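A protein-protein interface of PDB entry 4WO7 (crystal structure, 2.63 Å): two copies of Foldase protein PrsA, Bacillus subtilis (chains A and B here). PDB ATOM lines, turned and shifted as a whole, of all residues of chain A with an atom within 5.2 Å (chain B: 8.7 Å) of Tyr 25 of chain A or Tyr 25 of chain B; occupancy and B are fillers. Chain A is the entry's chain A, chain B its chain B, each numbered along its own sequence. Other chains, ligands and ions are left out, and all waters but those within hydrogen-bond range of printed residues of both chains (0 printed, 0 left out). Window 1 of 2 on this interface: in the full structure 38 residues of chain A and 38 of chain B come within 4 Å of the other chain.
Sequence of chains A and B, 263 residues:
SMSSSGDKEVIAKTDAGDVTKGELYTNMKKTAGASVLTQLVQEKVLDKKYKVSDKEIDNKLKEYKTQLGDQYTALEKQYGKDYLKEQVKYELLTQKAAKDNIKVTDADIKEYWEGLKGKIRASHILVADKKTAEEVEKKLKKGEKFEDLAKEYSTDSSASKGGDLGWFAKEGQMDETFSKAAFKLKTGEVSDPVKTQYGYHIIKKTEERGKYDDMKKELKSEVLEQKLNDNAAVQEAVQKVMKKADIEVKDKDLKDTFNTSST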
ATOM      1  N   GLU A   9      24.198  -6.241  17.207  1.00  0.00           N
ATOM      2  CA  GLU A   9      23.860  -5.489  18.408  1.00  0.00           C
ATOM      3  C   GLU A   9      24.044  -6.358  19.644  1.00  0.00           C
ATOM      4  O   GLU A   9      23.481  -7.449  19.744  1.00  0.00           O
ATOM      5  CB  GLU A   9      22.421  -4.971  18.309  1.00  0.00           C
ATOM      6  CG  GLU A   9      21.920  -4.189  19.513  1.00  0.00           C
ATOM      7  CD  GLU A   9      20.410  -4.041  19.504  1.00  0.00           C
ATOM      8  OE1 GLU A   9      19.813  -3.945  20.597  1.00  0.00           O
ATOM      9  OE2 GLU A   9      19.821  -4.005  18.400  1.00  0.00           O
ATOM     10  N   ILE A  11      23.309  -7.538  23.122  1.00  0.00           N
ATOM     11  CA  ILE A  11      22.212  -7.533  24.076  1.00  0.00           C
ATOM     12  C   ILE A  11      22.761  -7.515  25.489  1.00  0.00           C
ATOM     13  O   ILE A  11      22.308  -6.746  26.341  1.00  0.00           O
ATOM     14  CB  ILE A  11      21.320  -8.778  23.918  1.00  0.00           C
ATOM     15  CG1 ILE A  11      20.726  -8.857  22.509  1.00  0.00           C
ATOM     16  CG2 ILE A  11      20.235  -8.809  25.001  1.00  0.00           C
ATOM     17  CD1 ILE A  11      19.801  -7.721  22.161  1.00  0.00           C
ATOM     18  N   THR A  20      24.581 -11.624  21.297  1.00  0.00           N
ATOM     19  CA  THR A  20      24.136 -10.696  20.265  1.00  0.00           C
ATOM     20  C   THR A  20      22.627 -10.788  20.020  1.00  0.00           C
ATOM     21  O   THR A  20      21.977 -11.751  20.429  1.00  0.00           O
ATOM     22  CB  THR A  20      24.873 -10.954  18.945  1.00  0.00           C
ATOM     23  OG1 THR A  20      24.621 -12.294  18.507  1.00  0.00           O
ATOM     24  CG2 THR A  20      26.377 -10.736  19.117  1.00  0.00           C
ATOM     25  N   LYS A  21      22.085  -9.777  19.346  1.00  0.00           N
ATOM     26  CA  LYS A  21      20.674  -9.749  18.952  1.00  0.00           C
ATOM     27  C   LYS A  21      20.322 -10.968  18.102  1.00  0.00           C
ATOM     28  O   LYS A  21      19.267 -11.578  18.282  1.00  0.00           O
ATOM     29  CB  LYS A  21      20.366  -8.454  18.186  1.00  0.00           C
ATOM     30  CG  LYS A  21      18.962  -8.355  17.587  1.00  0.00           C
ATOM     31  CD  LYS A  21      18.587  -6.895  17.298  1.00  0.00           C
ATOM     32  CE  LYS A  21      17.472  -6.795  16.263  1.00  0.00           C
ATOM     33  NZ  LYS A  21      16.911  -5.419  16.137  1.00  0.00           N
ATOM     34  N   GLY A  22      21.214 -11.319  17.179  1.00  0.00           N
ATOM     35  CA  GLY A  22      21.005 -12.458  16.301  1.00  0.00           C
ATOM     36  C   GLY A  22      20.896 -13.767  17.064  1.00  0.00           C
ATOM     37  O   GLY A  22      20.044 -14.606  16.767  1.00  0.00           O
ATOM     38  N   GLU A  23      21.762 -13.941  18.056  1.00  0.00           N
ATOM     39  CA  GLU A  23      21.717 -15.124  18.905  1.00  0.00           C
ATOM     40  C   GLU A  23      20.393 -15.191  19.643  1.00  0.00           C
ATOM     41  O   GLU A  23      19.764 -16.247  19.712  1.00  0.00           O
ATOM     42  CB  GLU A  23      22.863 -15.114  19.920  1.00  0.00           C
ATOM     43  CG  GLU A  23      24.245 -15.321  19.330  1.00  0.00           C
ATOM     44  CD  GLU A  23      25.344 -15.043  20.339  1.00  0.00           C
ATOM     45  OE1 GLU A  23      25.720 -15.975  21.078  1.00  0.00           O
ATOM     46  OE2 GLU A  23      25.830 -13.891  20.393  1.00  0.00           O
ATOM     47  N   LEU A  24      19.972 -14.051  20.183  1.00  0.00           N
ATOM     48  CA  LEU A  24      18.723 -13.972  20.924  1.00  0.00           C
ATOM     49  C   LEU A  24      17.550 -14.308  20.012  1.00  0.00           C
ATOM     50  O   LEU A  24      16.692 -15.120  20.348  1.00  0.00           O
ATOM     51  CB  LEU A  24      18.543 -12.569  21.518  1.00  0.00           C
ATOM     52  CG  LEU A  24      17.364 -12.372  22.474  1.00  0.00           C
ATOM     53  CD1 LEU A  24      17.570 -13.189  23.734  1.00  0.00           C
ATOM     54  CD2 LEU A  24      17.158 -10.897  22.809  1.00  0.00           C
ATOM     55  N   TYR A  25      17.541 -13.702  18.831  1.00  0.00           N
ATOM     56  CA  TYR A  25      16.482 -13.947  17.863  1.00  0.00           C
ATOM     57  C   TYR A  25      16.394 -15.421  17.462  1.00  0.00           C
ATOM     58  O   TYR A  25      15.308 -15.997  17.451  1.00  0.00           O
ATOM     59  CB  TYR A  25      16.686 -13.094  16.612  1.00  0.00           C
ATOM     60  CG  TYR A  25      15.637 -13.343  15.550  1.00  0.00           C
ATOM     61  CD1 TYR A  25      14.348 -12.843  15.696  1.00  0.00           C
ATOM     62  CD2 TYR A  25      15.930 -14.069  14.402  1.00  0.00           C
ATOM     63  CE1 TYR A  25      13.384 -13.064  14.735  1.00  0.00           C
ATOM     64  CE2 TYR A  25      14.967 -14.291  13.434  1.00  0.00           C
ATOM     65  CZ  TYR A  25      13.696 -13.787  13.605  1.00  0.00           C
ATOM     66  OH  TYR A  25      12.729 -14.004  12.649  1.00  0.00           O
ATOM     67  N   THR A  26      17.536 -16.033  17.144  1.00  0.00           N
ATOM     68  CA  THR A  26      17.568 -17.437  16.708  1.00  0.00           C
ATOM     69  C   THR A  26      17.010 -18.396  17.758  1.00  0.00           C
ATOM     70  O   THR A  26      16.181 -19.254  17.449  1.00  0.00           O
ATOM     71  CB  THR A  26      19.008 -17.892  16.353  1.00  0.00           C
ATOM     72  OG1 THR A  26      19.449 -17.229  15.163  1.00  0.00           O
ATOM     73  CG2 THR A  26      19.086 -19.417  16.136  1.00  0.00           C
ATOM     74  N   ASN A  27      17.451 -18.239  19.000  1.00  0.00           N
ATOM     75  CA  ASN A  27      17.052 -19.151  20.068  1.00  0.00           C
ATOM     76  C   ASN A  27      15.633 -18.901  20.529  1.00  0.00           C
ATOM     77  O   ASN A  27      14.945 -19.825  20.957  1.00  0.00           O
ATOM     78  CB  ASN A  27      18.008 -19.032  21.252  1.00  0.00           C
ATOM     79  CG  ASN A  27      19.336 -19.696  20.985  1.00  0.00           C
ATOM     80  OD1 ASN A  27      19.506 -20.889  21.236  1.00  0.00           O
ATOM     81  ND2 ASN A  27      20.282 -18.933  20.446  1.00  0.00           N
ATOM     82  N   MET A  28      15.193 -17.653  20.439  1.00  0.00           N
ATOM     83  CA  MET A  28      13.814 -17.317  20.759  1.00  0.00           C
ATOM     84  C   MET A  28      12.871 -18.000  19.789  1.00  0.00           C
ATOM     85  O   MET A  28      11.774 -18.423  20.155  1.00  0.00           O
ATOM     86  CB  MET A  28      13.609 -15.806  20.712  1.00  0.00           C
ATOM     87  CG  MET A  28      14.165 -15.117  21.926  1.00  0.00           C
ATOM     88  SD  MET A  28      13.621 -13.252  22.099  1.00  0.00           S
ATOM     89  CE  MET A  28      12.360 -13.750  23.410  1.00  0.00           C
ATOM     90  N   LYS A  29      13.320 -18.118  18.547  1.00  0.00           N
ATOM     91  CA  LYS A  29      12.465 -18.603  17.477  1.00  0.00           C
ATOM     92  C   LYS A  29      12.215 -20.105  17.609  1.00  0.00           C
ATOM     93  O   LYS A  29      11.129 -20.592  17.290  1.00  0.00           O
ATOM     94  CB  LYS A  29      13.084 -18.295  16.120  1.00  0.00           C
ATOM     95  CG  LYS A  29      12.083 -18.372  14.990  1.00  0.00           C
ATOM     96  CD  LYS A  29      12.629 -17.749  13.727  1.00  0.00           C
ATOM     97  CE  LYS A  29      12.968 -18.827  12.719  1.00  0.00           C
ATOM     98  NZ  LYS A  29      13.692 -18.292  11.541  1.00  0.00           N
ATOM     99  N   ASP A 251       8.809 -18.084   6.236  1.00  0.00           N
ATOM    100  CA  ASP A 251       9.959 -18.598   6.967  1.00  0.00           C
ATOM    101  C   ASP A 251       9.861 -20.116   7.050  1.00  0.00           C
ATOM    102  O   ASP A 251       8.909 -20.646   7.621  1.00  0.00           O
ATOM    103  CB  ASP A 251      10.017 -17.971   8.366  1.00  0.00           C
ATOM    104  CG  ASP A 251      11.297 -18.302   9.109  1.00  0.00           C
ATOM    105  OD1 ASP A 251      11.359 -19.377   9.738  1.00  0.00           O
ATOM    106  OD2 ASP A 251      12.237 -17.478   9.075  1.00  0.00           O
ATOM    107  N   GLY B   6      16.545  -6.404   6.402  1.00  0.00           N
ATOM    108  CA  GLY B   6      16.873  -7.099   7.633  1.00  0.00           C
ATOM    109  C   GLY B   6      15.640  -7.437   8.445  1.00  0.00           C
ATOM    110  O   GLY B   6      14.989  -8.457   8.217  1.00  0.00           O
ATOM    111  N   ASP B   7      15.321  -6.571   9.401  1.00  0.00           N
ATOM    112  CA  ASP B   7      14.134  -6.734  10.236  1.00  0.00           C
ATOM    113  C   ASP B   7      12.817  -6.529   9.475  1.00  0.00           C
ATOM    114  O   ASP B   7      11.752  -6.896   9.971  1.00  0.00           O
ATOM    115  CB  ASP B   7      14.212  -5.786  11.438  1.00  0.00           C
ATOM    116  CG  ASP B   7      15.067  -6.346  12.568  1.00  0.00           C
ATOM    117  OD1 ASP B   7      15.929  -7.209  12.298  1.00  0.00           O
ATOM    118  OD2 ASP B   7      14.871  -5.928  13.729  1.00  0.00           O
ATOM    119  N   GLU B   9      12.228  -8.073   6.768  1.00  0.00           N
ATOM    120  CA  GLU B   9      11.981  -9.389   6.171  1.00  0.00           C
ATOM    121  C   GLU B   9      10.616  -9.946   6.585  1.00  0.00           C
ATOM    122  O   GLU B   9      10.271  -9.963   7.767  1.00  0.00           O
ATOM    123  CB  GLU B   9      13.081 -10.376   6.573  1.00  0.00           C
ATOM    124  CG  GLU B   9      12.877 -11.803   6.062  1.00  0.00           C
ATOM    125  CD  GLU B   9      13.745 -12.807   6.796  1.00  0.00           C
ATOM    126  OE1 GLU B   9      14.851 -12.429   7.236  1.00  0.00           O
ATOM    127  OE2 GLU B   9      13.318 -13.971   6.944  1.00  0.00           O
ATOM    128  N   VAL B  10       9.847 -10.404   5.602  1.00  0.00           N
ATOM    129  CA  VAL B  10       8.506 -10.938   5.845  1.00  0.00           C
ATOM    130  C   VAL B  10       8.531 -12.387   6.334  1.00  0.00           C
ATOM    131  O   VAL B  10       8.990 -13.278   5.618  1.00  0.00           O
ATOM    132  CB  VAL B  10       7.641 -10.854   4.563  1.00  0.00           C
ATOM    133  CG1 VAL B  10       6.304 -11.582   4.742  1.00  0.00           C
ATOM    134  CG2 VAL B  10       7.412  -9.399   4.179  1.00  0.00           C
ATOM    135  N   ILE B  11       8.038 -12.608   7.552  1.00  0.00           N
ATOM    136  CA  ILE B  11       7.927 -13.953   8.117  1.00  0.00           C
ATOM    137  C   ILE B  11       6.663 -14.645   7.630  1.00  0.00           C
ATOM    138  O   ILE B  11       6.688 -15.810   7.231  1.00  0.00           O
ATOM    139  CB  ILE B  11       7.909 -13.928   9.665  1.00  0.00           C
ATOM    140  CG1 ILE B  11       9.212 -13.333  10.206  1.00  0.00           C
ATOM    141  CG2 ILE B  11       7.645 -15.338  10.242  1.00  0.00           C
ATOM    142  CD1 ILE B  11      10.443 -14.136   9.853  1.00  0.00           C
ATOM    143  N   VAL B  19       3.633 -10.128   8.772  1.00  0.00           N
ATOM    144  CA  VAL B  19       4.422 -10.133  10.002  1.00  0.00           C
ATOM    145  C   VAL B  19       5.892 -10.091   9.623  1.00  0.00           C
ATOM    146  O   VAL B  19       6.376 -10.957   8.901  1.00  0.00           O
ATOM    147  CB  VAL B  19       4.157 -11.379  10.889  1.00  0.00           C
ATOM    148  CG1 VAL B  19       5.134 -11.439  12.083  1.00  0.00           C
ATOM    149  CG2 VAL B  19       2.712 -11.403  11.363  1.00  0.00           C
ATOM    150  N   THR B  20       6.587  -9.068  10.104  1.00  0.00           N
ATOM    151  CA  THR B  20       8.001  -8.889   9.823  1.00  0.00           C
ATOM    152  C   THR B  20       8.873  -9.549  10.874  1.00  0.00           C
ATOM    153  O   THR B  20       8.417  -9.871  11.970  1.00  0.00           O
ATOM    154  CB  THR B  20       8.380  -7.396   9.750  1.00  0.00           C
ATOM    155  OG1 THR B  20       7.987  -6.740  10.964  1.00  0.00           O
ATOM    156  CG2 THR B  20       7.709  -6.723   8.565  1.00  0.00           C
ATOM    157  N   LYS B  21      10.137  -9.740  10.514  1.00  0.00           N
ATOM    158  CA  LYS B  21      11.141 -10.255  11.428  1.00  0.00           C
ATOM    159  C   LYS B  21      11.286  -9.370  12.656  1.00  0.00           C
ATOM    160  O   LYS B  21      11.375  -9.860  13.783  1.00  0.00           O
ATOM    161  CB  LYS B  21      12.486 -10.379  10.710  1.00  0.00           C
ATOM    162  CG  LYS B  21      13.649 -10.701  11.634  1.00  0.00           C
ATOM    163  CD  LYS B  21      14.824 -11.328  10.896  1.00  0.00           C
ATOM    164  CE  LYS B  21      16.113 -11.151  11.691  1.00  0.00           C
ATOM    165  NZ  LYS B  21      17.239 -11.989  11.185  1.00  0.00           N
ATOM    166  N   GLY B  22      11.320  -8.062  12.425  1.00  0.00           N
ATOM    167  CA  GLY B  22      11.461  -7.099  13.500  1.00  0.00           C
ATOM    168  C   GLY B  22      10.283  -7.163  14.444  1.00  0.00           C
ATOM    169  O   GLY B  22      10.451  -7.140  15.664  1.00  0.00           O
ATOM    170  N   GLU B  23       9.079  -7.267  13.881  1.00  0.00           N
ATOM    171  CA  GLU B  23       7.875  -7.372  14.711  1.00  0.00           C
ATOM    172  C   GLU B  23       7.945  -8.632  15.552  1.00  0.00           C
ATOM    173  O   GLU B  23       7.636  -8.614  16.745  1.00  0.00           O
ATOM    174  CB  GLU B  23       6.563  -7.413  13.899  1.00  0.00           C
ATOM    175  CG  GLU B  23       5.298  -7.438  14.794  1.00  0.00           C
ATOM    176  CD  GLU B  23       4.010  -7.863  14.100  1.00  0.00           C
ATOM    177  OE1 GLU B  23       2.928  -7.334  14.516  1.00  0.00           O
ATOM    178  OE2 GLU B  23       4.094  -8.678  13.141  1.00  0.00           O
ATOM    179  N   LEU B  24       8.324  -9.733  14.912  1.00  0.00           N
ATOM    180  CA  LEU B  24       8.442 -11.013  15.594  1.00  0.00           C
ATOM    181  C   LEU B  24       9.507 -10.974  16.671  1.00  0.00           C
ATOM    182  O   LEU B  24       9.294 -11.446  17.786  1.00  0.00           O
ATOM    183  CB  LEU B  24       8.759 -12.119  14.600  1.00  0.00           C
ATOM    184  CG  LEU B  24       8.792 -13.514  15.220  1.00  0.00           C
ATOM    185  CD1 LEU B  24       7.428 -13.931  15.748  1.00  0.00           C
ATOM    186  CD2 LEU B  24       9.310 -14.506  14.194  1.00  0.00           C
ATOM    187  N   TYR B  25      10.657 -10.408  16.331  1.00  0.00           N
ATOM    188  CA  TYR B  25      11.728 -10.253  17.299  1.00  0.00           C
ATOM    189  C   TYR B  25      11.247  -9.489  18.519  1.00  0.00           C
ATOM    190  O   TYR B  25      11.513  -9.876  19.655  1.00  0.00           O
ATOM    191  CB  TYR B  25      12.914  -9.524  16.681  1.00  0.00           C
ATOM    192  CG  TYR B  25      13.954  -9.140  17.703  1.00  0.00           C
ATOM    193  CD1 TYR B  25      14.805 -10.081  18.255  1.00  0.00           C
ATOM    194  CD2 TYR B  25      14.072  -7.824  18.126  1.00  0.00           C
ATOM    195  CE1 TYR B  25      15.751  -9.719  19.205  1.00  0.00           C
ATOM    196  CE2 TYR B  25      15.008  -7.456  19.068  1.00  0.00           C
ATOM    197  CZ  TYR B  25      15.844  -8.405  19.605  1.00  0.00           C
ATOM    198  OH  TYR B  25      16.781  -8.035  20.539  1.00  0.00           O
ATOM    199  N   THR B  26      10.546  -8.394  18.269  1.00  0.00           N
ATOM    200  CA  THR B  26      10.026  -7.563  19.343  1.00  0.00           C
ATOM    201  C   THR B  26       9.067  -8.306  20.276  1.00  0.00           C
ATOM    202  O   THR B  26       9.210  -8.251  21.496  1.00  0.00           O
ATOM    203  CB  THR B  26       9.304  -6.317  18.772  1.00  0.00           C
ATOM    204  OG1 THR B  26      10.269  -5.403  18.233  1.00  0.00           O
ATOM    205  CG2 THR B  26       8.492  -5.596  19.850  1.00  0.00           C
ATOM    206  N   ASN B  27       8.101  -9.015  19.705  1.00  0.00           N
ATOM    207  CA  ASN B  27       7.085  -9.673  20.525  1.00  0.00           C
ATOM    208  C   ASN B  27       7.558 -10.946  21.219  1.00  0.00           C
ATOM    209  O   ASN B  27       7.016 -11.318  22.260  1.00  0.00           O
ATOM    210  CB  ASN B  27       5.845  -9.974  19.683  1.00  0.00           C
ATOM    211  CG  ASN B  27       5.005  -8.738  19.442  1.00  0.00           C
ATOM    212  OD1 ASN B  27       4.131  -8.409  20.247  1.00  0.00           O
ATOM    213  ND2 ASN B  27       5.280  -8.031  18.353  1.00  0.00           N
ATOM    214  N   MET B  28       8.559 -11.617  20.659  1.00  0.00           N
ATOM    215  CA  MET B  28       9.181 -12.707  21.382  1.00  0.00           C
ATOM    216  C   MET B  28       9.883 -12.111  22.612  1.00  0.00           C
ATOM    217  O   MET B  28       9.754 -12.639  23.718  1.00  0.00           O
ATOM    218  CB  MET B  28      10.159 -13.488  20.494  1.00  0.00           C
ATOM    219  CG  MET B  28       9.463 -14.348  19.440  1.00  0.00           C
ATOM    220  SD  MET B  28      10.595 -15.535  18.389  1.00  0.00           S
ATOM    221  CE  MET B  28      11.776 -14.262  17.525  1.00  0.00           C
ATOM    222  N   LYS B  29      10.569 -10.980  22.420  1.00  0.00           N
ATOM    223  CA  LYS B  29      11.425 -10.386  23.455  1.00  0.00           C
ATOM    224  C   LYS B  29      10.625 -10.083  24.714  1.00  0.00           C
ATOM    225  O   LYS B  29      11.130 -10.219  25.829  1.00  0.00           O
ATOM    226  CB  LYS B  29      12.115  -9.124  22.919  1.00  0.00           C
ATOM    227  CG  LYS B  29      13.320  -8.662  23.753  1.00  0.00           C
ATOM    228  CD  LYS B  29      14.252  -7.730  22.970  1.00  0.00           C
ATOM    229  CE  LYS B  29      14.184  -6.270  23.401  1.00  0.00           C
ATOM    230  NZ  LYS B  29      12.896  -5.604  23.076  1.00  0.00           N
ATOM    231  N   LYS B  30       9.377  -9.678  24.525  1.00  0.00           N
ATOM    232  CA  LYS B  30       8.504  -9.335  25.633  1.00  0.00           C
ATOM    233  C   LYS B  30       8.069 -10.577  26.408  1.00  0.00           C
ATOM    234  O   LYS B  30       7.887 -10.508  27.621  1.00  0.00           O
ATOM    235  CB  LYS B  30       7.285  -8.566  25.112  1.00  0.00           C
ATOM    236  CG  LYS B  30       7.598  -7.143  24.633  1.00  0.00           C
ATOM    237  CD  LYS B  30       6.494  -6.602  23.734  1.00  0.00           C
ATOM    238  CE  LYS B  30       6.805  -5.191  23.270  1.00  0.00           C
ATOM    239  NZ  LYS B  30       5.939  -4.743  22.145  1.00  0.00           N
ATOM    240  N   THR B  31       7.923 -11.710  25.726  1.00  0.00           N
ATOM    241  CA  THR B  31       7.400 -12.913  26.364  1.00  0.00           C
ATOM    242  C   THR B  31       8.542 -13.781  26.895  1.00  0.00           C
ATOM    243  O   THR B  31       8.527 -14.214  28.046  1.00  0.00           O
ATOM    244  CB  THR B  31       6.555 -13.745  25.390  1.00  0.00           C
ATOM    245  OG1 THR B  31       5.655 -12.886  24.679  1.00  0.00           O
ATOM    246  CG2 THR B  31       5.775 -14.828  26.140  1.00  0.00           C
ATOM    247  N   ALA B  32       9.538 -14.007  26.041  1.00  0.00           N
ATOM    248  CA  ALA B  32      10.551 -15.035  26.260  1.00  0.00           C
ATOM    249  C   ALA B  32      11.978 -14.480  26.345  1.00  0.00           C
ATOM    250  O   ALA B  32      12.926 -15.236  26.548  1.00  0.00           O
ATOM    251  CB  ALA B  32      10.463 -16.068  25.132  1.00  0.00           C
ATOM    252  N   GLY B  33      12.131 -13.167  26.186  1.00  0.00           N
ATOM    253  CA  GLY B  33      13.450 -12.555  26.135  1.00  0.00           C
ATOM    254  C   GLY B  33      14.309 -12.812  27.356  1.00  0.00           C
ATOM    255  O   GLY B  33      15.479 -13.176  27.239  1.00  0.00           O
ATOM    256  N   VAL B  36      15.220 -16.734  27.714  1.00  0.00           N
ATOM    257  CA  VAL B  36      16.174 -17.223  26.719  1.00  0.00           C
ATOM    258  C   VAL B  36      17.530 -16.540  26.851  1.00  0.00           C
ATOM    259  O   VAL B  36      18.560 -17.187  26.683  1.00  0.00           O
ATOM    260  CB  VAL B  36      15.638 -17.040  25.281  1.00  0.00           C
ATOM    261  CG1 VAL B  36      16.739 -17.280  24.235  1.00  0.00           C
ATOM    262  CG2 VAL B  36      14.442 -17.957  25.050  1.00  0.00           C
ATOM    263  N   LEU B  37      17.538 -15.248  27.166  1.00  0.00           N
ATOM    264  CA  LEU B  37      18.786 -14.555  27.475  1.00  0.00           C
ATOM    265  C   LEU B  37      19.476 -15.190  28.678  1.00  0.00           C
ATOM    266  O   LEU B  37      20.702 -15.285  28.720  1.00  0.00           O
ATOM    267  CB  LEU B  37      18.530 -13.072  27.747  1.00  0.00           C
ATOM    268  CG  LEU B  37      19.747 -12.231  28.150  1.00  0.00           C
ATOM    269  CD1 LEU B  37      20.824 -12.198  27.066  1.00  0.00           C
ATOM    270  CD2 LEU B  37      19.291 -10.827  28.509  1.00  0.00           C
ATOM    271  N   LEU B  40      21.222 -18.395  27.473  1.00  0.00           N
ATOM    272  CA  LEU B  40      22.349 -18.045  26.611  1.00  0.00           C
ATOM    273  C   LEU B  40      23.550 -17.583  27.436  1.00  0.00           C
ATOM    274  O   LEU B  40      24.682 -17.992  27.178  1.00  0.00           O
ATOM    275  CB  LEU B  40      21.938 -16.956  25.615  1.00  0.00           C
ATOM    276  CG  LEU B  40      20.957 -17.392  24.522  1.00  0.00           C
ATOM    277  CD1 LEU B  40      20.456 -16.176  23.757  1.00  0.00           C
ATOM    278  CD2 LEU B  40      21.583 -18.403  23.563  1.00  0.00           C
ATOM    279  N   ASP B 251      20.644  -4.033  26.862  1.00  0.00           N
ATOM    280  CA  ASP B 251      19.304  -3.829  26.302  1.00  0.00           C
ATOM    281  C   ASP B 251      18.330  -3.236  27.325  1.00  0.00           C
ATOM    282  O   ASP B 251      18.168  -3.754  28.430  1.00  0.00           O
ATOM    283  CB  ASP B 251      18.728  -5.135  25.761  1.00  0.00           C
ATOM    284  CG  ASP B 251      17.466  -4.916  24.945  1.00  0.00           C
ATOM    285  OD1 ASP B 251      16.372  -4.829  25.543  1.00  0.00           O
ATOM    286  OD2 ASP B 251      17.571  -4.821  23.704  1.00  0.00           O
ATOM    287  N   ASP B 253      14.953  -2.950  27.518  1.00  0.00           N
ATOM    288  CA  ASP B 253      13.779  -3.718  27.924  1.00  0.00           C
ATOM    289  C   ASP B 253      14.112  -4.842  28.900  1.00  0.00           C
ATOM    290  O   ASP B 253      13.276  -5.228  29.715  1.00  0.00           O
ATOM    291  CB  ASP B 253      13.079  -4.290  26.690  1.00  0.00           C
ATOM    292  CG  ASP B 253      12.750  -3.221  25.663  1.00  0.00           C
ATOM    293  OD1 ASP B 253      11.733  -2.516  25.843  1.00  0.00           O
ATOM    294  OD2 ASP B 253      13.504  -3.085  24.676  1.00  0.00           O
ATOM    295  N   LEU B 254      15.338  -5.352  28.806  1.00  0.00           N
ATOM    296  CA  LEU B 254      15.776  -6.536  29.546  1.00  0.00           C
ATOM    297  C   LEU B 254      16.761  -6.220  30.667  1.00  0.00           C
ATOM    298  O   LEU B 254      17.409  -7.122  31.198  1.00  0.00           O
ATOM    299  CB  LEU B 254      16.425  -7.527  28.581  1.00  0.00           C
ATOM    300  CG  LEU B 254      15.542  -8.103  27.478  1.00  0.00           C
ATOM    301  CD1 LEU B 254      16.418  -8.696  26.393  1.00  0.00           C
ATOM    302  CD2 LEU B 254      14.609  -9.163  28.051  1.00  0.00           C
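Among the printed residues, merely in contact across the chains: Glu 9 of chain A with Asp 251 of chain B, Ile 11 of chain A with Tyr 25 of chain B, Lys 21 of chain A with Tyr 25 of chain B, Leu 24 of chain A with Tyr 25 of chain B, Leu 24 of chain A with Leu 40 of chain B, Tyr 25 of chain A with Ile 11 of chain B, Tyr 25 of chain A with Lys 21 of chain B, Tyr 25 of chain A with Leu 24 of chain B, Tyr 25 of chain A with Tyr 25 of chain B, Tyr 25 of chain A with Met 28 of chain B, Asn 27 of chain A with Val 36 of chain B, Asn 27 of chain A with Leu 40 of chain B, Met 28 of chain A with Lys 29 of chain B, Met 28 of chain A with Ala 32 of chain B and Met 28 of chain A with Gly 33 of chain B.
The side-chain amino group (NZ) of Lys 29 of chain B lies within salt-bridge range of the side-chain carboxylate (OD2) of Asp 253 of chain B, at 3.0 Å.
N of Lys 21 of chain B lies within hydrogen-bond range of O of Asp 7 of chain B, 3.3 Å away.
NZ of Lys 29 of chain A lies within salt-bridge range of OD2 of Asp 251 of chain A (3.0 Å).
Printed residues of chain A that touch a printed residue of chain B: Glu 9, Ile 11, Lys 21, Leu 24, Tyr 25, Asn 27, Met 28, Lys 29 and Asp 251.
Hydrophobic or aromatic side chains of chain A that line the printed part of chain B: Ile 11, Leu 24, Tyr 25 and Met 28.
Of the 26 printed residues of chain B, 12 touch a printed residue of chain A.
Printed residues of chain B that touch a printed residue of chain A: Asp 7, Ile 11, Lys 21, Leu 24, Tyr 25, Met 28, Lys 29, Ala 32, Gly 33, Val 36, Leu 40 and Asp 251.
Thr 20 of chain A touches none of the printed residues of chain B.
Printed residues of chain B within 4 Å of Tyr 25 of chain A: Ile 11, Lys 21, Leu 24, Tyr 25 and Met 28.
Printed residues of chain A within 4 Å of Leu 24 of chain B: Tyr 25.
Of the printed residues of chain A, Met 28 of chain B touches Tyr 25 (3.4 Å), Met 28 (2.8 Å) and Lys 29 (3.7 Å).
The nearest residue of chain A that does not touch Tyr 25 of chain B is Met 28 of chain A (4.7 Å).
Ile 11 of chain A touches Asp 251 of chain B, and with the chains exchanged Asp 251 of chain A touches Ile 11 of chain B.
Leu 24 of chain A touches Tyr 25 of chain B, and with the chains exchanged Tyr 25 of chain A touches Leu 24 of chain B.
Positions printed for both chains: 9, 11, 20, 21, 22, 23, 24, 25, 26, 27, 28, 29 and 251.
Of the 20 pairs that touch across the chains among the printed residues, 12 have their exchanged pair printed and touching as well.
The backbone NH of Asp 251 of chain A sits at hydrogen-bond distance from the backbone carbonyl oxygen of Ile 11 of chain B (3.3 Å).
O of Ile 11 of chain A lies within hydrogen-bond range of N of Asp 251 of chain B.
The side-chain amino group (NZ) of Lys 21 of chain A is in salt-bridge range of the side-chain carboxylate (OD2) of Asp 7 of chain B (3.2 Å).
O of Met 28 of chain A lies close to SD of Met 28 of chain B.
The backbone NH of Lys 29 of chain A sits close to the side-chain sulfur of Met 28 of chain B, at 3.8 Å.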
